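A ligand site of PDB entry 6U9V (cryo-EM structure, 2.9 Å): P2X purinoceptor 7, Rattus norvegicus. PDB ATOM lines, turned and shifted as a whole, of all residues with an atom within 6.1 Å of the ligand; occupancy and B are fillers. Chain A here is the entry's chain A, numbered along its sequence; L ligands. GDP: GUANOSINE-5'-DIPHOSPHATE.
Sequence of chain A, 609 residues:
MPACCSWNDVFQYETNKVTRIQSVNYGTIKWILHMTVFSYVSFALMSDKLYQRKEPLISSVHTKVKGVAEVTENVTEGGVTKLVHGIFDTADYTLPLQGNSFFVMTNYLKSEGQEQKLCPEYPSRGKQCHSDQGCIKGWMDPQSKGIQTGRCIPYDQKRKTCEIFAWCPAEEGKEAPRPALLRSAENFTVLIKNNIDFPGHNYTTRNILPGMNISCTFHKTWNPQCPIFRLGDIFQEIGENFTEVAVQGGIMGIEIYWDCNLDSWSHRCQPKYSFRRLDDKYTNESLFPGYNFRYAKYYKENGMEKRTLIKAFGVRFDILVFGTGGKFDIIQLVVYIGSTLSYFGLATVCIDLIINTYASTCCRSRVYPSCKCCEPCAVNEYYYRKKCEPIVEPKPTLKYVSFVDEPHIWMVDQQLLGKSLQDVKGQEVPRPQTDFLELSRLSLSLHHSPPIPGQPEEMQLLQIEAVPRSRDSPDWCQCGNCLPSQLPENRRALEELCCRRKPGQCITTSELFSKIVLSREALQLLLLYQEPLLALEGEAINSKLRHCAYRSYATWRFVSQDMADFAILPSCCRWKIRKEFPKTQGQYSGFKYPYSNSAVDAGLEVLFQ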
ATOM      1  N   GLU A 495      29.009  13.187 -24.580  1.00  0.00           N
ATOM      2  CA  GLU A 495      28.314  13.042 -25.860  1.00  0.00           C
ATOM      3  C   GLU A 495      28.157  14.382 -26.571  1.00  0.00           C
ATOM      4  O   GLU A 495      27.729  14.407 -27.733  1.00  0.00           O
ATOM      5  CB  GLU A 495      26.944  12.402 -25.641  1.00  0.00           C
ATOM      6  CG  GLU A 495      26.946  11.075 -24.878  1.00  0.00           C
ATOM      7  CD  GLU A 495      27.631   9.948 -25.638  1.00  0.00           C
ATOM      8  OE1 GLU A 495      28.840  10.056 -25.923  1.00  0.00           O
ATOM      9  OE2 GLU A 495      26.942   8.943 -25.941  1.00  0.00           O
ATOM     10  N   SER A 543      21.244  -4.703 -30.608  1.00  0.00           N
ATOM     11  CA  SER A 543      22.375  -4.211 -29.814  1.00  0.00           C
ATOM     12  C   SER A 543      23.701  -4.506 -30.497  1.00  0.00           C
ATOM     13  O   SER A 543      24.579  -3.634 -30.581  1.00  0.00           O
ATOM     14  CB  SER A 543      22.336  -4.831 -28.418  1.00  0.00           C
ATOM     15  OG  SER A 543      23.426  -4.388 -27.632  1.00  0.00           O
ATOM     16  N   ARG A 546      24.102  -2.287 -33.482  1.00  0.00           N
ATOM     17  CA  ARG A 546      24.443  -0.923 -33.100  1.00  0.00           C
ATOM     18  C   ARG A 546      25.919  -0.827 -32.721  1.00  0.00           C
ATOM     19  O   ARG A 546      26.616   0.123 -33.095  1.00  0.00           O
ATOM     20  CB  ARG A 546      23.564  -0.467 -31.937  1.00  0.00           C
ATOM     21  CG  ARG A 546      23.133   0.986 -32.023  1.00  0.00           C
ATOM     22  CD  ARG A 546      22.387   1.445 -30.771  1.00  0.00           C
ATOM     23  NE  ARG A 546      21.298   0.547 -30.388  1.00  0.00           N
ATOM     24  CZ  ARG A 546      21.383  -0.449 -29.508  1.00  0.00           C
ATOM     25  NH1 ARG A 546      22.513  -0.729 -28.870  1.00  0.00           N
ATOM     26  NH2 ARG A 546      20.311  -1.180 -29.247  1.00  0.00           N
ATOM     27  N   HIS A 547      26.416  -1.816 -31.955  1.00  0.00           N
ATOM     28  CA  HIS A 547      27.825  -1.818 -31.582  1.00  0.00           C
ATOM     29  C   HIS A 547      28.717  -1.939 -32.810  1.00  0.00           C
ATOM     30  O   HIS A 547      29.744  -1.258 -32.912  1.00  0.00           O
ATOM     31  CB  HIS A 547      28.105  -2.965 -30.611  1.00  0.00           C
ATOM     32  CG  HIS A 547      27.292  -2.915 -29.356  1.00  0.00           C
ATOM     33  ND1 HIS A 547      27.216  -3.972 -28.466  1.00  0.00           N
ATOM     34  CD2 HIS A 547      26.514  -1.930 -28.831  1.00  0.00           C
ATOM     35  CE1 HIS A 547      26.433  -3.639 -27.463  1.00  0.00           C
ATOM     36  NE2 HIS A 547      25.994  -2.408 -27.656  1.00  0.00           N
ATOM     37  N   TYR A 550      28.792   1.396 -34.600  1.00  0.00           N
ATOM     38  CA  TYR A 550      29.722   2.299 -33.915  1.00  0.00           C
ATOM     39  C   TYR A 550      31.156   1.962 -34.289  1.00  0.00           C
ATOM     40  O   TYR A 550      31.958   2.851 -34.620  1.00  0.00           O
ATOM     41  CB  TYR A 550      29.530   2.215 -32.395  1.00  0.00           C
ATOM     42  CG  TYR A 550      28.167   2.635 -31.877  1.00  0.00           C
ATOM     43  CD1 TYR A 550      27.317   3.454 -32.612  1.00  0.00           C
ATOM     44  CD2 TYR A 550      27.743   2.232 -30.612  1.00  0.00           C
ATOM     45  CE1 TYR A 550      26.084   3.844 -32.125  1.00  0.00           C
ATOM     46  CE2 TYR A 550      26.516   2.602 -30.117  1.00  0.00           C
ATOM     47  CZ  TYR A 550      25.691   3.418 -30.872  1.00  0.00           C
ATOM     48  OH  TYR A 550      24.464   3.788 -30.376  1.00  0.00           O
ATOM     49  N   ARG A 551      31.511   0.670 -34.239  1.00  0.00           N
ATOM     50  CA  ARG A 551      32.868   0.257 -34.605  1.00  0.00           C
ATOM     51  C   ARG A 551      33.161   0.564 -36.065  1.00  0.00           C
ATOM     52  O   ARG A 551      34.297   0.920 -36.412  1.00  0.00           O
ATOM     53  CB  ARG A 551      33.057  -1.235 -34.335  1.00  0.00           C
ATOM     54  CG  ARG A 551      33.241  -1.576 -32.867  1.00  0.00           C
ATOM     55  CD  ARG A 551      33.449  -3.063 -32.645  1.00  0.00           C
ATOM     56  NE  ARG A 551      34.614  -3.576 -33.367  1.00  0.00           N
ATOM     57  CZ  ARG A 551      35.877  -3.400 -32.997  1.00  0.00           C
ATOM     58  NH1 ARG A 551      36.858  -3.914 -33.732  1.00  0.00           N
ATOM     59  NH2 ARG A 551      36.192  -2.711 -31.904  1.00  0.00           N
ATOM     60  N   ALA A 554      33.849   4.242 -36.369  1.00  0.00           N
ATOM     61  CA  ALA A 554      35.152   4.504 -35.753  1.00  0.00           C
ATOM     62  C   ALA A 554      36.285   4.121 -36.685  1.00  0.00           C
ATOM     63  O   ALA A 554      37.188   4.922 -36.949  1.00  0.00           O
ATOM     64  CB  ALA A 554      35.270   3.758 -34.427  1.00  0.00           C
ATOM     65  N   ALA A 564      40.424   3.915 -33.222  1.00  0.00           N
ATOM     66  CA  ALA A 564      39.014   3.545 -33.311  1.00  0.00           C
ATOM     67  C   ALA A 564      38.419   3.346 -31.923  1.00  0.00           C
ATOM     68  O   ALA A 564      37.339   3.869 -31.618  1.00  0.00           O
ATOM     69  CB  ALA A 564      38.843   2.293 -34.153  1.00  0.00           C
ATOM     70  N   ASP A 565      39.116   2.598 -31.070  1.00  0.00           N
ATOM     71  CA  ASP A 565      38.777   2.570 -29.657  1.00  0.00           C
ATOM     72  C   ASP A 565      39.046   3.942 -29.058  1.00  0.00           C
ATOM     73  O   ASP A 565      39.878   4.700 -29.557  1.00  0.00           O
ATOM     74  CB  ASP A 565      39.578   1.500 -28.930  1.00  0.00           C
ATOM     75  CG  ASP A 565      39.344   0.111 -29.491  1.00  0.00           C
ATOM     76  OD1 ASP A 565      38.226  -0.156 -29.970  1.00  0.00           O
ATOM     77  OD2 ASP A 565      40.281  -0.719 -29.447  1.00  0.00           O
ATOM     78  N   PHE A 566      38.318   4.278 -27.994  1.00  0.00           N
ATOM     79  CA  PHE A 566      38.398   5.585 -27.343  1.00  0.00           C
ATOM     80  C   PHE A 566      37.973   6.713 -28.275  1.00  0.00           C
ATOM     81  O   PHE A 566      38.379   7.862 -28.073  1.00  0.00           O
ATOM     82  CB  PHE A 566      39.801   5.853 -26.807  1.00  0.00           C
ATOM     83  CG  PHE A 566      40.358   4.736 -25.982  1.00  0.00           C
ATOM     84  CD1 PHE A 566      39.967   4.559 -24.667  1.00  0.00           C
ATOM     85  CD2 PHE A 566      41.260   3.843 -26.533  1.00  0.00           C
ATOM     86  CE1 PHE A 566      40.478   3.526 -23.921  1.00  0.00           C
ATOM     87  CE2 PHE A 566      41.780   2.810 -25.782  1.00  0.00           C
ATOM     88  CZ  PHE A 566      41.381   2.643 -24.474  1.00  0.00           C
ATOM     89  N   ALA A 567      37.161   6.422 -29.284  1.00  0.00           N
ATOM     90  CA  ALA A 567      36.619   7.430 -30.181  1.00  0.00           C
ATOM     91  C   ALA A 567      35.233   7.837 -29.700  1.00  0.00           C
ATOM     92  O   ALA A 567      34.473   7.017 -29.181  1.00  0.00           O
ATOM     93  CB  ALA A 567      36.538   6.903 -31.612  1.00  0.00           C
ATOM     94  N   ILE A 568      34.903   9.124 -29.877  1.00  0.00           N
ATOM     95  CA  ILE A 568      33.628   9.687 -29.478  1.00  0.00           C
ATOM     96  C   ILE A 568      32.890  10.100 -30.746  1.00  0.00           C
ATOM     97  O   ILE A 568      33.335  10.995 -31.463  1.00  0.00           O
ATOM     98  CB  ILE A 568      33.801  10.881 -28.530  1.00  0.00           C
ATOM     99  CG1 ILE A 568      34.709  10.522 -27.338  1.00  0.00           C
ATOM    100  CG2 ILE A 568      32.446  11.398 -28.045  1.00  0.00           C
ATOM    101  CD1 ILE A 568      34.258   9.304 -26.530  1.00  0.00           C
ATOM    102  N   LEU A 569      31.770   9.434 -31.011  1.00  0.00           N
ATOM    103  CA  LEU A 569      31.001   9.744 -32.212  1.00  0.00           C
ATOM    104  C   LEU A 569      30.201  11.029 -31.988  1.00  0.00           C
ATOM    105  O   LEU A 569      29.910  11.382 -30.841  1.00  0.00           O
ATOM    106  CB  LEU A 569      30.054   8.597 -32.558  1.00  0.00           C
ATOM    107  CG  LEU A 569      30.600   7.170 -32.447  1.00  0.00           C
ATOM    108  CD1 LEU A 569      29.613   6.197 -33.062  1.00  0.00           C
ATOM    109  CD2 LEU A 569      31.959   7.048 -33.095  1.00  0.00           C
ATOM    110  N   ARG A 574      25.451   9.390 -33.933  1.00  0.00           N
ATOM    111  CA  ARG A 574      25.093   8.491 -32.843  1.00  0.00           C
ATOM    112  C   ARG A 574      23.586   8.250 -32.810  1.00  0.00           C
ATOM    113  O   ARG A 574      23.121   7.107 -32.797  1.00  0.00           O
ATOM    114  CB  ARG A 574      25.576   9.066 -31.512  1.00  0.00           C
ATOM    115  CG  ARG A 574      25.438   8.126 -30.317  1.00  0.00           C
ATOM    116  CD  ARG A 574      25.738   8.858 -29.023  1.00  0.00           C
ATOM    117  NE  ARG A 574      27.079   9.436 -28.998  1.00  0.00           N
ATOM    118  CZ  ARG A 574      28.199   8.775 -28.711  1.00  0.00           C
ATOM    119  NH1 ARG A 574      29.357   9.409 -28.719  1.00  0.00           N
ATOM    120  NH2 ARG A 574      28.179   7.480 -28.403  1.00  0.00           N
ATOM    121  N   ARG A 578      21.244   5.022 -33.592  1.00  0.00           N
ATOM    122  CA  ARG A 578      20.287   4.558 -32.590  1.00  0.00           C
ATOM    123  C   ARG A 578      18.870   4.507 -33.167  1.00  0.00           C
ATOM    124  O   ARG A 578      18.084   3.619 -32.824  1.00  0.00           O
ATOM    125  CB  ARG A 578      20.335   5.457 -31.355  1.00  0.00           C
ATOM    126  CG  ARG A 578      21.596   5.290 -30.537  1.00  0.00           C
ATOM    127  CD  ARG A 578      21.701   6.323 -29.428  1.00  0.00           C
ATOM    128  NE  ARG A 578      22.869   6.074 -28.575  1.00  0.00           N
ATOM    129  CZ  ARG A 578      23.204   6.809 -27.513  1.00  0.00           C
ATOM    130  NH1 ARG A 578      24.279   6.488 -26.808  1.00  0.00           N
ATOM    131  NH2 ARG A 578      22.467   7.847 -27.126  1.00  0.00           N
ATOM    132  N   LYS A 583      16.635   0.837 -29.040  1.00  0.00           N
ATOM    133  CA  LYS A 583      16.590  -0.006 -27.845  1.00  0.00           C
ATOM    134  C   LYS A 583      15.228   0.176 -27.195  1.00  0.00           C
ATOM    135  O   LYS A 583      14.844   1.302 -26.852  1.00  0.00           O
ATOM    136  CB  LYS A 583      17.712   0.365 -26.871  1.00  0.00           C
ATOM    137  CG  LYS A 583      17.880  -0.615 -25.720  1.00  0.00           C
ATOM    138  CD  LYS A 583      19.084  -0.261 -24.869  1.00  0.00           C
ATOM    139  CE  LYS A 583      19.316  -1.292 -23.777  1.00  0.00           C
ATOM    140  NZ  LYS A 583      20.478  -0.945 -22.917  1.00  0.00           N
ATOM    141  N   GLN A 587      17.757   2.433 -21.518  1.00  0.00           N
ATOM    142  CA  GLN A 587      18.481   3.616 -21.957  1.00  0.00           C
ATOM    143  C   GLN A 587      19.762   3.209 -22.677  1.00  0.00           C
ATOM    144  O   GLN A 587      20.253   2.089 -22.550  1.00  0.00           O
ATOM    145  CB  GLN A 587      18.804   4.508 -20.756  1.00  0.00           C
ATOM    146  CG  GLN A 587      17.597   5.008 -19.987  1.00  0.00           C
ATOM    147  CD  GLN A 587      16.726   5.950 -20.803  1.00  0.00           C
ATOM    148  OE1 GLN A 587      17.122   6.407 -21.864  1.00  0.00           O
ATOM    149  NE2 GLN A 587      15.534   6.241 -20.285  1.00  0.00           N
ATOM    150  N   TYR A 588      20.301   4.144 -23.446  1.00  0.00           N
ATOM    151  CA  TYR A 588      21.509   3.923 -24.242  1.00  0.00           C
ATOM    152  C   TYR A 588      22.726   4.265 -23.393  1.00  0.00           C
ATOM    153  O   TYR A 588      22.950   5.439 -23.062  1.00  0.00           O
ATOM    154  CB  TYR A 588      21.494   4.751 -25.510  1.00  0.00           C
ATOM    155  CG  TYR A 588      20.324   4.458 -26.432  1.00  0.00           C
ATOM    156  CD1 TYR A 588      20.363   3.383 -27.305  1.00  0.00           C
ATOM    157  CD2 TYR A 588      19.198   5.253 -26.427  1.00  0.00           C
ATOM    158  CE1 TYR A 588      19.304   3.104 -28.142  1.00  0.00           C
ATOM    159  CE2 TYR A 588      18.127   4.995 -27.264  1.00  0.00           C
ATOM    160  CZ  TYR A 588      18.190   3.910 -28.119  1.00  0.00           C
ATOM    161  OH  TYR A 588      17.132   3.641 -28.957  1.00  0.00           O
ATOM    162  N   SER A 589      23.520   3.254 -23.055  1.00  0.00           N
ATOM    163  CA  SER A 589      24.757   3.482 -22.321  1.00  0.00           C
ATOM    164  C   SER A 589      25.819   4.038 -23.267  1.00  0.00           C
ATOM    165  O   SER A 589      26.098   3.464 -24.318  1.00  0.00           O
ATOM    166  CB  SER A 589      25.249   2.187 -21.683  1.00  0.00           C
ATOM    167  OG  SER A 589      26.424   2.400 -20.929  1.00  0.00           O
ATOM    168  N   GLY A 590      26.412   5.168 -22.877  1.00  0.00           N
ATOM    169  CA  GLY A 590      27.391   5.833 -23.700  1.00  0.00           C
ATOM    170  C   GLY A 590      28.698   5.071 -23.781  1.00  0.00           C
ATOM    171  O   GLY A 590      28.777   3.863 -23.554  1.00  0.00           O
ATOM    172  N   PHE A 591      29.757   5.815 -24.114  1.00  0.00           N
ATOM    173  CA  PHE A 591      31.080   5.231 -24.224  1.00  0.00           C
ATOM    174  C   PHE A 591      31.561   4.730 -22.872  1.00  0.00           C
ATOM    175  O   PHE A 591      31.412   5.413 -21.859  1.00  0.00           O
ATOM    176  CB  PHE A 591      32.062   6.255 -24.794  1.00  0.00           C
ATOM    177  CG  PHE A 591      33.506   5.877 -24.622  1.00  0.00           C
ATOM    178  CD1 PHE A 591      34.077   4.901 -25.431  1.00  0.00           C
ATOM    179  CD2 PHE A 591      34.289   6.487 -23.653  1.00  0.00           C
ATOM    180  CE1 PHE A 591      35.397   4.548 -25.273  1.00  0.00           C
ATOM    181  CE2 PHE A 591      35.615   6.132 -23.503  1.00  0.00           C
ATOM    182  CZ  PHE A 591      36.173   5.168 -24.311  1.00  0.00           C
ATOM    183  N   LYS A 592      32.132   3.523 -22.861  1.00  0.00           N
ATOM    184  CA  LYS A 592      32.645   2.883 -21.662  1.00  0.00           C
ATOM    185  C   LYS A 592      34.088   2.481 -21.887  1.00  0.00           C
ATOM    186  O   LYS A 592      34.463   2.097 -22.998  1.00  0.00           O
ATOM    187  CB  LYS A 592      31.811   1.657 -21.291  1.00  0.00           C
ATOM    188  CG  LYS A 592      30.383   1.987 -20.888  1.00  0.00           C
ATOM    189  CD  LYS A 592      29.641   0.780 -20.312  1.00  0.00           C
ATOM    190  CE  LYS A 592      29.437  -0.330 -21.342  1.00  0.00           C
ATOM    191  NZ  LYS A 592      30.535  -1.334 -21.335  1.00  0.00           N
HETATM  192  PB  GDP L   1      23.727  -0.260 -24.588  1.00  0.00           P
HETATM  193  O1B GDP L   1      22.431  -0.496 -25.323  1.00  0.00           O
HETATM  194  O2B GDP L   1      23.475  -0.304 -23.090  1.00  0.00           O
HETATM  195  O3B GDP L   1      24.726  -1.320 -24.954  1.00  0.00           O
HETATM  196  O3A GDP L   1      24.327   1.225 -24.996  1.00  0.00           O
HETATM  197  PA  GDP L   1      24.764   1.638 -26.532  1.00  0.00           P
HETATM  198  O1A GDP L   1      23.778   1.038 -27.505  1.00  0.00           O
HETATM  199  O2A GDP L   1      24.766   3.133 -26.675  1.00  0.00           O
HETATM  200  O5' GDP L   1      26.267   1.050 -26.860  1.00  0.00           O
HETATM  201  C5' GDP L   1      27.142   0.779 -25.800  1.00  0.00           C
HETATM  202  C4' GDP L   1      28.267  -0.093 -26.326  1.00  0.00           C
HETATM  203  O4' GDP L   1      28.861   0.574 -27.673  1.00  0.00           O
HETATM  204  C3' GDP L   1      29.246  -0.190 -25.464  1.00  0.00           C
HETATM  205  O3' GDP L   1      29.830  -1.565 -25.504  1.00  0.00           O
HETATM  206  C2' GDP L   1      30.303   0.834 -25.912  1.00  0.00           C
HETATM  207  O2' GDP L   1      31.551   0.339 -25.696  1.00  0.00           O
HETATM  208  C1' GDP L   1      30.065   1.033 -27.420  1.00  0.00           C
HETATM  209  N9  GDP L   1      30.162   2.457 -27.792  1.00  0.00           N
HETATM  210  C8  GDP L   1      29.017   3.109 -27.537  1.00  0.00           C
HETATM  211  N7  GDP L   1      29.201   4.390 -27.890  1.00  0.00           N
HETATM  212  C5  GDP L   1      30.437   4.524 -28.380  1.00  0.00           C
HETATM  213  C6  GDP L   1      31.203   5.722 -28.938  1.00  0.00           C
HETATM  214  O6  GDP L   1      30.677   6.781 -28.994  1.00  0.00           O
HETATM  215  N1  GDP L   1      32.546   5.571 -29.399  1.00  0.00           N
HETATM  216  C2  GDP L   1      33.182   4.278 -29.320  1.00  0.00           C
HETATM  217  N2  GDP L   1      34.539   4.116 -29.783  1.00  0.00           N
HETATM  218  N3  GDP L   1      32.444   3.136 -28.788  1.00  0.00           N
HETATM  219  C4  GDP L   1      31.045   3.301 -28.317  1.00  0.00           C
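An oxygen (O1A) of the ligand is in salt-bridge range of the guanidinium group of Arg 546 (2.6 Å).
A ring nitrogen (NE2) of His 547 sits at hydrogen-bond distance from an oxygen (O3B) of the ligand.
An oxygen (O2B) of the ligand lies within salt-bridge range of the side-chain amino group of Lys 583 (3.1 Å).
The backbone carbonyl oxygen of Ala 564 sits at hydrogen-bond distance from a nitrogen (N2) of the ligand (3.4 Å).
O of Ser 589 lies close to O2A of the ligand (2.7 Å).
N of Ser 589 sits at hydrogen-bond distance from O3A of the ligand (2.9 Å).
The guanidinium group (NH2) of Arg 574 lies within hydrogen-bond range of an oxygen (O6) of the ligand, at 2.7 Å.
An oxygen (O2A) of the ligand is in salt-bridge range of the guanidinium group (NH1) of Arg 578, 3.4 Å away.
O of Ala 567 sits at hydrogen-bond distance from N1 of the ligand (2.4 Å).
The backbone NH (N) of Lys 583 lies within hydrogen-bond range of the side-chain hydroxyl (OH) of Tyr 588 (2.8 Å).
O of Leu 569 lies within hydrogen-bond range of NH1 of Arg 574 (2.9 Å).
The guanidinium group (NH1) of Arg 578 lies within salt-bridge range of the side-chain carboxylate (OE2) of Glu 495.
OE1 of Glu 495 is in salt-bridge range of NH1 of Arg 574 (2.9 Å).
NE of Arg 578 lies close to OH of Tyr 550, 3.3 Å away.
The side-chain hydroxyl (OG) of Ser 543 sits close to a ring nitrogen (NE2) of His 547 (3.2 Å).
The side-chain amino group (NZ) of Lys 583 is in hydrogen-bond range of the backbone carbonyl oxygen (O) of Gln 587 (3.1 Å).
CD2 of Tyr 550 touches C8 of the ligand, 3.4 Å away.
CG of Leu 569 touches O6 of the ligand, at 3.5 Å.
Tyr 588 touches the ligand (C to O3A, 3.8 Å).
Hydrophobic or aromatic side chains that line the ligand: His 547, Tyr 550, Ala 567, Leu 569 and Tyr 588.
Within 4 Å of the ligand: Arg 546, His 547, Tyr 550, Ala 564, Ala 567, Leu 569, Arg 574, Arg 578, Lys 583, Tyr 588 and Ser 589.
The nearest printed residue that does not touch the ligand is Phe 591 (4.04 Å).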
